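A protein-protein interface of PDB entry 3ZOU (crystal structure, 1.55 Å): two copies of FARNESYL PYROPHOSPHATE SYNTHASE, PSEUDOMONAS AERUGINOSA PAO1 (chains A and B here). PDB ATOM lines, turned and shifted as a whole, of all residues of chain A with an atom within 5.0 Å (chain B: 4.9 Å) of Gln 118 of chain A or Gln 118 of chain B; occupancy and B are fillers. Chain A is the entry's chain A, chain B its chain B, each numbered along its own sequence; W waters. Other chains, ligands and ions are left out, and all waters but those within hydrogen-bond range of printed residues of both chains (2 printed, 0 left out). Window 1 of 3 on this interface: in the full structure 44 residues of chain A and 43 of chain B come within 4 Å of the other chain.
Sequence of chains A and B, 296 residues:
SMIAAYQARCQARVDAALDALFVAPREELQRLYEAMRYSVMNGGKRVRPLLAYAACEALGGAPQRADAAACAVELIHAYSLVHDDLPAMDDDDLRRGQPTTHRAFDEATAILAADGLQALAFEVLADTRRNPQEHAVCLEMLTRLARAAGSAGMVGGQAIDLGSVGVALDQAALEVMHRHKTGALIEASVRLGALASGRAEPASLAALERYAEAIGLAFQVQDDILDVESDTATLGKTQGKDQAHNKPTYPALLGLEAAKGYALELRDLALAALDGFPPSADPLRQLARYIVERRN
The side-chain amide nitrogen (NE2) of Gln 118 of chain A sits at hydrogen-bond distance from the backbone carbonyl oxygen (O) of Asp 115 of chain B (3.3 Å). The backbone carbonyl oxygen of Asp 115 of chain A is in hydrogen-bond range of the side-chain amide nitrogen of Gln 118 of chain B, at 3.2 Å.
Among the printed residues, merely in contact across the chains: Tyr 79 of chain A with Asp 115 of chain B (3.3 Å), Asp 115 of chain A with Tyr 79 of chain B (3.3 Å), Asp 115 of chain A with Asp 115 of chain B (3.5 Å), Gln 118 of chain A with Gln 118 of chain B (3.5 Å), Gln 118 of chain A with Ala 119 of chain B (3.4 Å), Ala 119 of chain A with Gln 118 of chain B (3.4 Å) and Phe 122 of chain A with Phe 122 of chain B (3.4 Å).
Printed residues of chain B within 4 Å of Tyr 79 of chain A: Asp 115 (3.3 Å). Gln 118 of chain A touches just these residues of chain B: Asp 115, Gln 118 and Ala 119. Of the printed residues of chain B, Ala 119 of chain A touches Gln 118 (3.4 Å). Of the printed residues of chain A, Tyr 79 of chain B touches Asp 115. Printed residues of chain A within 4 Å of Asp 115 of chain B: Tyr 79, Asp 115 and Gln 118. Gln 118 of chain B touches just these residues of chain A: Asp 115, Gln 118 and Ala 119. Of the printed residues of chain A, Ala 119 of chain B touches Gln 118 (3.4 Å). The nearest printed residue of chain B that does not touch Gln 118 of chain A is Phe 122 of chain B (5.2 Å). The nearest printed residue of chain A that does not touch Gln 118 of chain B is Phe 122 of chain A (5.2 Å). The nearest printed residue of chain B that does not touch Asp 115 of chain A is Ala 149 of chain B (5.8 Å).
Printed residues of chain B that touch a printed residue of chain A: Tyr 79, Asp 115, Gln 118, Ala 119 and Phe 122. Of the 12 printed residues of chain A, 5 touch a printed residue of chain B. Printed residues of chain A that touch a printed residue of chain B: Tyr 79, Asp 115, Gln 118, Ala 119 and Phe 122. Among the printed residues, no Asp or Glu carboxylate lies within 4 Å of a Lys or Arg side-chain nitrogen of the other chain.
Tyr 79 of chain A touches Asp 115 of chain B, and with the chains exchanged Asp 115 of chain A touches Tyr 79 of chain B. Asp 115 of chain A touches Gln 118 of chain B, and with the chains exchanged Gln 118 of chain A touches Asp 115 of chain B. Gln 118 of chain A touches Ala 119 of chain B, and with the chains exchanged Ala 119 of chain A touches Gln 118 of chain B. Phe 122 of chain B touches its own counterpart, Phe 122 of chain A. Of the 9 pairs that touch across the chains among the printed residues, 9 have their exchanged pair printed and touching as well.
Water W2 lies within hydrogen-bond range of the side-chain carboxylate (OD1) of Asp 115 of chain B (2.8 Å), the side-chain carboxylate (OD1) of Asp 115 of chain A (2.8 Å), the side-chain amide nitrogen (NE2) of Gln 118 of chain A (3.0 Å) and the side-chain amide nitrogen (NE2) of Gln 118 of chain B (3.0 Å). Water W1 bridges the side-chain hydroxyl of Tyr 79 of chain B and the side-chain carboxylate of Asp 115 of chain A.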
ATOM      1  N   ILE A  76      29.600   0.689 -21.896  1.00  0.00           N
ATOM      2  CA  ILE A  76      28.302   1.310 -21.664  1.00  0.00           C
ATOM      3  C   ILE A  76      28.494   2.490 -20.660  1.00  0.00           C
ATOM      4  O   ILE A  76      27.903   3.581 -20.791  1.00  0.00           O
ATOM      5  CB  ILE A  76      27.243   0.308 -21.179  1.00  0.00           C
ATOM      6  CG1 ILE A  76      26.913  -0.739 -22.269  1.00  0.00           C
ATOM      7  CG2 ILE A  76      25.965   1.015 -20.680  1.00  0.00           C
ATOM      8  CD1 ILE A  76      26.315  -0.157 -23.527  1.00  0.00           C
ATOM      9  N   TYR A  79      30.156   5.497 -22.278  1.00  0.00           N
ATOM     10  CA  TYR A  79      29.312   6.241 -23.261  1.00  0.00           C
ATOM     11  C   TYR A  79      28.309   7.077 -22.437  1.00  0.00           C
ATOM     12  O   TYR A  79      28.057   8.266 -22.769  1.00  0.00           O
ATOM     13  CB  TYR A  79      28.625   5.364 -24.287  1.00  0.00           C
ATOM     14  CG  TYR A  79      27.098   5.270 -24.154  1.00  0.00           C
ATOM     15  CD1 TYR A  79      26.314   6.325 -24.521  1.00  0.00           C
ATOM     16  CD2 TYR A  79      26.455   4.141 -23.705  1.00  0.00           C
ATOM     17  CE1 TYR A  79      24.929   6.275 -24.390  1.00  0.00           C
ATOM     18  CE2 TYR A  79      25.078   4.084 -23.547  1.00  0.00           C
ATOM     19  CZ  TYR A  79      24.317   5.136 -23.904  1.00  0.00           C
ATOM     20  OH  TYR A  79      22.973   5.083 -23.722  1.00  0.00           O
ATOM     21  N   ALA A 114      30.442   8.540 -28.294  1.00  0.00           N
ATOM     22  CA  ALA A 114      29.654   7.782 -27.311  1.00  0.00           C
ATOM     23  C   ALA A 114      28.643   6.861 -27.953  1.00  0.00           C
ATOM     24  O   ALA A 114      28.478   5.690 -27.548  1.00  0.00           O
ATOM     25  CB  ALA A 114      29.035   8.703 -26.312  1.00  0.00           C
ATOM     26  N   ASP A 115      27.978   7.275 -29.031  1.00  0.00           N
ATOM     27  CA  ASP A 115      27.098   6.361 -29.757  1.00  0.00           C
ATOM     28  C   ASP A 115      27.872   5.121 -30.284  1.00  0.00           C
ATOM     29  O   ASP A 115      27.305   4.016 -30.247  1.00  0.00           O
ATOM     30  CB  ASP A 115      26.456   7.100 -30.944  1.00  0.00           C
ATOM     31  CG  ASP A 115      25.389   8.076 -30.564  1.00  0.00           C
ATOM     32  OD1 ASP A 115      24.853   8.053 -29.468  1.00  0.00           O
ATOM     33  OD2 ASP A 115      25.023   8.950 -31.438  1.00  0.00           O
ATOM     34  N   GLY A 116      29.094   5.322 -30.791  1.00  0.00           N
ATOM     35  CA  GLY A 116      29.926   4.258 -31.276  1.00  0.00           C
ATOM     36  C   GLY A 116      30.390   3.352 -30.130  1.00  0.00           C
ATOM     37  O   GLY A 116      30.542   2.166 -30.340  1.00  0.00           O
ATOM     38  N   LEU A 117      30.581   3.910 -28.931  1.00  0.00           N
ATOM     39  CA  LEU A 117      30.952   3.086 -27.756  1.00  0.00           C
ATOM     40  C   LEU A 117      29.805   2.179 -27.421  1.00  0.00           C
ATOM     41  O   LEU A 117      30.018   1.049 -27.023  1.00  0.00           O
ATOM     42  CB  LEU A 117      31.333   3.976 -26.556  1.00  0.00           C
ATOM     43  CG  LEU A 117      32.656   4.748 -26.681  1.00  0.00           C
ATOM     44  CD1 LEU A 117      32.783   5.733 -25.536  1.00  0.00           C
ATOM     45  CD2 LEU A 117      33.833   3.843 -26.803  1.00  0.00           C
ATOM     46  N   GLN A 118      28.569   2.679 -27.495  1.00  0.00           N
ATOM     47  CA  GLN A 118      27.442   1.804 -27.188  1.00  0.00           C
ATOM     48  C   GLN A 118      27.379   0.617 -28.139  1.00  0.00           C
ATOM     49  O   GLN A 118      27.219  -0.522 -27.753  1.00  0.00           O
ATOM     50  CB  GLN A 118      26.109   2.555 -27.106  1.00  0.00           C
ATOM     51  CG  GLN A 118      25.006   1.561 -26.794  1.00  0.00           C
ATOM     52  CD  GLN A 118      23.645   2.109 -26.357  1.00  0.00           C
ATOM     53  OE1 GLN A 118      22.909   1.369 -25.720  1.00  0.00           O
ATOM     54  NE2 GLN A 118      23.258   3.251 -26.813  1.00  0.00           N
ATOM     55  N   ALA A 119      27.466   0.906 -29.451  1.00  0.00           N
ATOM     56  CA  ALA A 119      27.487  -0.213 -30.441  1.00  0.00           C
ATOM     57  C   ALA A 119      28.636  -1.184 -30.175  1.00  0.00           C
ATOM     58  O   ALA A 119      28.405  -2.379 -30.249  1.00  0.00           O
ATOM     59  CB  ALA A 119      27.562   0.312 -31.862  1.00  0.00           C
ATOM     60  N   LEU A 120      29.768  -0.607 -29.823  1.00  0.00           N
ATOM     61  CA  LEU A 120      30.928  -1.479 -29.582  1.00  0.00           C
ATOM     62  C   LEU A 120      30.683  -2.428 -28.446  1.00  0.00           C
ATOM     63  O   LEU A 120      31.197  -3.548 -28.444  1.00  0.00           O
ATOM     64  CB  LEU A 120      32.136  -0.648 -29.369  1.00  0.00           C
ATOM     65  CG  LEU A 120      33.487  -1.321 -29.157  1.00  0.00           C
ATOM     66  CD1 LEU A 120      33.795  -2.147 -30.373  1.00  0.00           C
ATOM     67  CD2 LEU A 120      34.534  -0.235 -28.969  1.00  0.00           C
ATOM     68  N   ALA A 121      30.029  -1.963 -27.392  1.00  0.00           N
ATOM     69  CA  ALA A 121      29.751  -2.807 -26.226  1.00  0.00           C
ATOM     70  C   ALA A 121      29.059  -4.087 -26.706  1.00  0.00           C
ATOM     71  O   ALA A 121      29.328  -5.206 -26.236  1.00  0.00           O
ATOM     72  CB  ALA A 121      28.948  -2.082 -25.189  1.00  0.00           C
ATOM     73  N   PHE A 122      28.049  -3.927 -27.552  1.00  0.00           N
ATOM     74  CA  PHE A 122      27.223  -5.037 -28.059  1.00  0.00           C
ATOM     75  C   PHE A 122      28.014  -5.886 -29.061  1.00  0.00           C
ATOM     76  O   PHE A 122      27.967  -7.110 -29.007  1.00  0.00           O
ATOM     77  CB  PHE A 122      25.870  -4.513 -28.618  1.00  0.00           C
ATOM     78  CG  PHE A 122      25.017  -3.920 -27.534  1.00  0.00           C
ATOM     79  CD1 PHE A 122      24.490  -4.736 -26.547  1.00  0.00           C
ATOM     80  CD2 PHE A 122      24.764  -2.590 -27.461  1.00  0.00           C
ATOM     81  CE1 PHE A 122      23.654  -4.186 -25.563  1.00  0.00           C
ATOM     82  CE2 PHE A 122      23.939  -2.044 -26.478  1.00  0.00           C
ATOM     83  CZ  PHE A 122      23.445  -2.844 -25.503  1.00  0.00           C
ATOM     84  N   ALA A 149      20.992  -1.401 -20.093  1.00  0.00           N
ATOM     85  CA  ALA A 149      21.566  -0.145 -20.625  1.00  0.00           C
ATOM     86  C   ALA A 149      20.447   0.758 -21.160  1.00  0.00           C
ATOM     87  O   ALA A 149      20.696   1.982 -21.259  1.00  0.00           O
ATOM     88  CB  ALA A 149      22.519  -0.407 -21.725  1.00  0.00           C
ATOM     89  N   ILE B  76      17.805   1.356 -35.329  1.00  0.00           N
ATOM     90  CA  ILE B  76      19.086   2.003 -35.606  1.00  0.00           C
ATOM     91  C   ILE B  76      18.938   3.275 -36.444  1.00  0.00           C
ATOM     92  O   ILE B  76      19.432   4.356 -36.114  1.00  0.00           O
ATOM     93  CB  ILE B  76      20.173   1.021 -36.200  1.00  0.00           C
ATOM     94  CG1 ILE B  76      20.492  -0.143 -35.186  1.00  0.00           C
ATOM     95  CG2 ILE B  76      21.423   1.786 -36.578  1.00  0.00           C
ATOM     96  CD1 ILE B  76      21.031   0.314 -33.856  1.00  0.00           C
ATOM     97  N   TYR B  79      17.210   6.059 -34.483  1.00  0.00           N
ATOM     98  CA  TYR B  79      18.021   6.702 -33.480  1.00  0.00           C
ATOM     99  C   TYR B  79      18.995   7.662 -34.159  1.00  0.00           C
ATOM    100  O   TYR B  79      19.269   8.738 -33.657  1.00  0.00           O
ATOM    101  CB  TYR B  79      18.722   5.671 -32.523  1.00  0.00           C
ATOM    102  CG  TYR B  79      20.224   5.649 -32.642  1.00  0.00           C
ATOM    103  CD1 TYR B  79      21.010   6.693 -32.124  1.00  0.00           C
ATOM    104  CD2 TYR B  79      20.908   4.611 -33.221  1.00  0.00           C
ATOM    105  CE1 TYR B  79      22.377   6.705 -32.256  1.00  0.00           C
ATOM    106  CE2 TYR B  79      22.268   4.576 -33.324  1.00  0.00           C
ATOM    107  CZ  TYR B  79      23.019   5.657 -32.865  1.00  0.00           C
ATOM    108  OH  TYR B  79      24.371   5.669 -33.092  1.00  0.00           O
ATOM    109  N   ALA B 114      16.931   8.345 -28.078  1.00  0.00           N
ATOM    110  CA  ALA B 114      17.669   7.718 -29.174  1.00  0.00           C
ATOM    111  C   ALA B 114      18.666   6.735 -28.585  1.00  0.00           C
ATOM    112  O   ALA B 114      18.877   5.676 -29.186  1.00  0.00           O
ATOM    113  CB  ALA B 114      18.247   8.761 -30.066  1.00  0.00           C
ATOM    114  N   ASP B 115      19.318   7.109 -27.494  1.00  0.00           N
ATOM    115  CA  ASP B 115      20.265   6.167 -26.863  1.00  0.00           C
ATOM    116  C   ASP B 115      19.491   4.872 -26.504  1.00  0.00           C
ATOM    117  O   ASP B 115      20.047   3.757 -26.680  1.00  0.00           O
ATOM    118  CB  ASP B 115      20.836   6.776 -25.604  1.00  0.00           C
ATOM    119  CG  ASP B 115      21.907   7.794 -25.839  1.00  0.00           C
ATOM    120  OD1 ASP B 115      22.461   7.884 -26.913  1.00  0.00           O
ATOM    121  OD2 ASP B 115      22.208   8.599 -24.869  1.00  0.00           O
ATOM    122  N   GLY B 116      18.271   5.001 -25.966  1.00  0.00           N
ATOM    123  CA  GLY B 116      17.415   3.871 -25.661  1.00  0.00           C
ATOM    124  C   GLY B 116      17.036   3.073 -26.896  1.00  0.00           C
ATOM    125  O   GLY B 116      16.862   1.846 -26.815  1.00  0.00           O
ATOM    126  N   LEU B 117      16.746   3.754 -28.019  1.00  0.00           N
ATOM    127  CA  LEU B 117      16.414   3.061 -29.258  1.00  0.00           C
ATOM    128  C   LEU B 117      17.572   2.181 -29.736  1.00  0.00           C
ATOM    129  O   LEU B 117      17.354   1.125 -30.296  1.00  0.00           O
ATOM    130  CB  LEU B 117      16.013   4.068 -30.360  1.00  0.00           C
ATOM    131  CG  LEU B 117      14.697   4.763 -30.167  1.00  0.00           C
ATOM    132  CD1 LEU B 117      14.554   5.832 -31.219  1.00  0.00           C
ATOM    133  CD2 LEU B 117      13.488   3.871 -30.144  1.00  0.00           C
ATOM    134  N   GLN B 118      18.799   2.671 -29.613  1.00  0.00           N
ATOM    135  CA  GLN B 118      19.936   1.869 -30.021  1.00  0.00           C
ATOM    136  C   GLN B 118      20.009   0.602 -29.174  1.00  0.00           C
ATOM    137  O   GLN B 118      20.170  -0.514 -29.722  1.00  0.00           O
ATOM    138  CB  GLN B 118      21.261   2.632 -30.002  1.00  0.00           C
ATOM    139  CG  GLN B 118      22.411   1.734 -30.435  1.00  0.00           C
ATOM    140  CD  GLN B 118      23.760   2.401 -30.733  1.00  0.00           C
ATOM    141  OE1 GLN B 118      24.477   1.750 -31.552  1.00  0.00           O
ATOM    142  NE2 GLN B 118      24.153   3.464 -30.203  1.00  0.00           N
ATOM    143  N   ALA B 119      19.908   0.746 -27.858  1.00  0.00           N
ATOM    144  CA  ALA B 119      19.958  -0.417 -27.015  1.00  0.00           C
ATOM    145  C   ALA B 119      18.846  -1.397 -27.426  1.00  0.00           C
ATOM    146  O   ALA B 119      19.046  -2.617 -27.428  1.00  0.00           O
ATOM    147  CB  ALA B 119      19.809  -0.131 -25.514  1.00  0.00           C
ATOM    148  N   LEU B 120      17.655  -0.890 -27.700  1.00  0.00           N
ATOM    149  CA  LEU B 120      16.538  -1.711 -28.018  1.00  0.00           C
ATOM    150  C   LEU B 120      16.733  -2.526 -29.287  1.00  0.00           C
ATOM    151  O   LEU B 120      16.235  -3.652 -29.413  1.00  0.00           O
ATOM    152  CB  LEU B 120      15.271  -0.835 -28.096  1.00  0.00           C
ATOM    153  CG  LEU B 120      13.942  -1.502 -28.405  1.00  0.00           C
ATOM    154  CD1 LEU B 120      13.597  -2.484 -27.305  1.00  0.00           C
ATOM    155  CD2 LEU B 120      12.877  -0.447 -28.469  1.00  0.00           C
ATOM    156  N   ALA B 121      17.413  -1.919 -30.256  1.00  0.00           N
ATOM    157  CA  ALA B 121      17.682  -2.617 -31.547  1.00  0.00           C
ATOM    158  C   ALA B 121      18.461  -3.919 -31.214  1.00  0.00           C
ATOM    159  O   ALA B 121      18.193  -4.981 -31.794  1.00  0.00           O
ATOM    160  CB  ALA B 121      18.509  -1.721 -32.449  1.00  0.00           C
ATOM    161  N   PHE B 122      19.411  -3.830 -30.286  1.00  0.00           N
ATOM    162  CA  PHE B 122      20.204  -5.019 -29.925  1.00  0.00           C
ATOM    163  C   PHE B 122      19.393  -5.975 -29.059  1.00  0.00           C
ATOM    164  O   PHE B 122      19.459  -7.198 -29.222  1.00  0.00           O
ATOM    165  CB  PHE B 122      21.523  -4.578 -29.316  1.00  0.00           C
ATOM    166  CG  PHE B 122      22.366  -3.838 -30.316  1.00  0.00           C
ATOM    167  CD1 PHE B 122      22.963  -4.525 -31.359  1.00  0.00           C
ATOM    168  CD2 PHE B 122      22.678  -2.502 -30.155  1.00  0.00           C
ATOM    169  CE1 PHE B 122      23.790  -3.865 -32.256  1.00  0.00           C
ATOM    170  CE2 PHE B 122      23.461  -1.836 -31.099  1.00  0.00           C
ATOM    171  CZ  PHE B 122      23.945  -2.510 -32.163  1.00  0.00           C
ATOM    172  N   ALA B 149      26.403  -0.367 -37.437  1.00  0.00           N
ATOM    173  CA  ALA B 149      25.881   0.816 -36.732  1.00  0.00           C
ATOM    174  C   ALA B 149      26.976   1.688 -36.099  1.00  0.00           C
ATOM    175  O   ALA B 149      26.722   2.852 -35.855  1.00  0.00           O
ATOM    176  CB  ALA B 149      24.884   0.408 -35.651  1.00  0.00           C
HETATM  177  O   HOH W   1      24.435   8.226 -34.591  1.00  0.00           O
HETATM  178  O   HOH W   2      23.648   5.777 -28.299  1.00  0.00           O
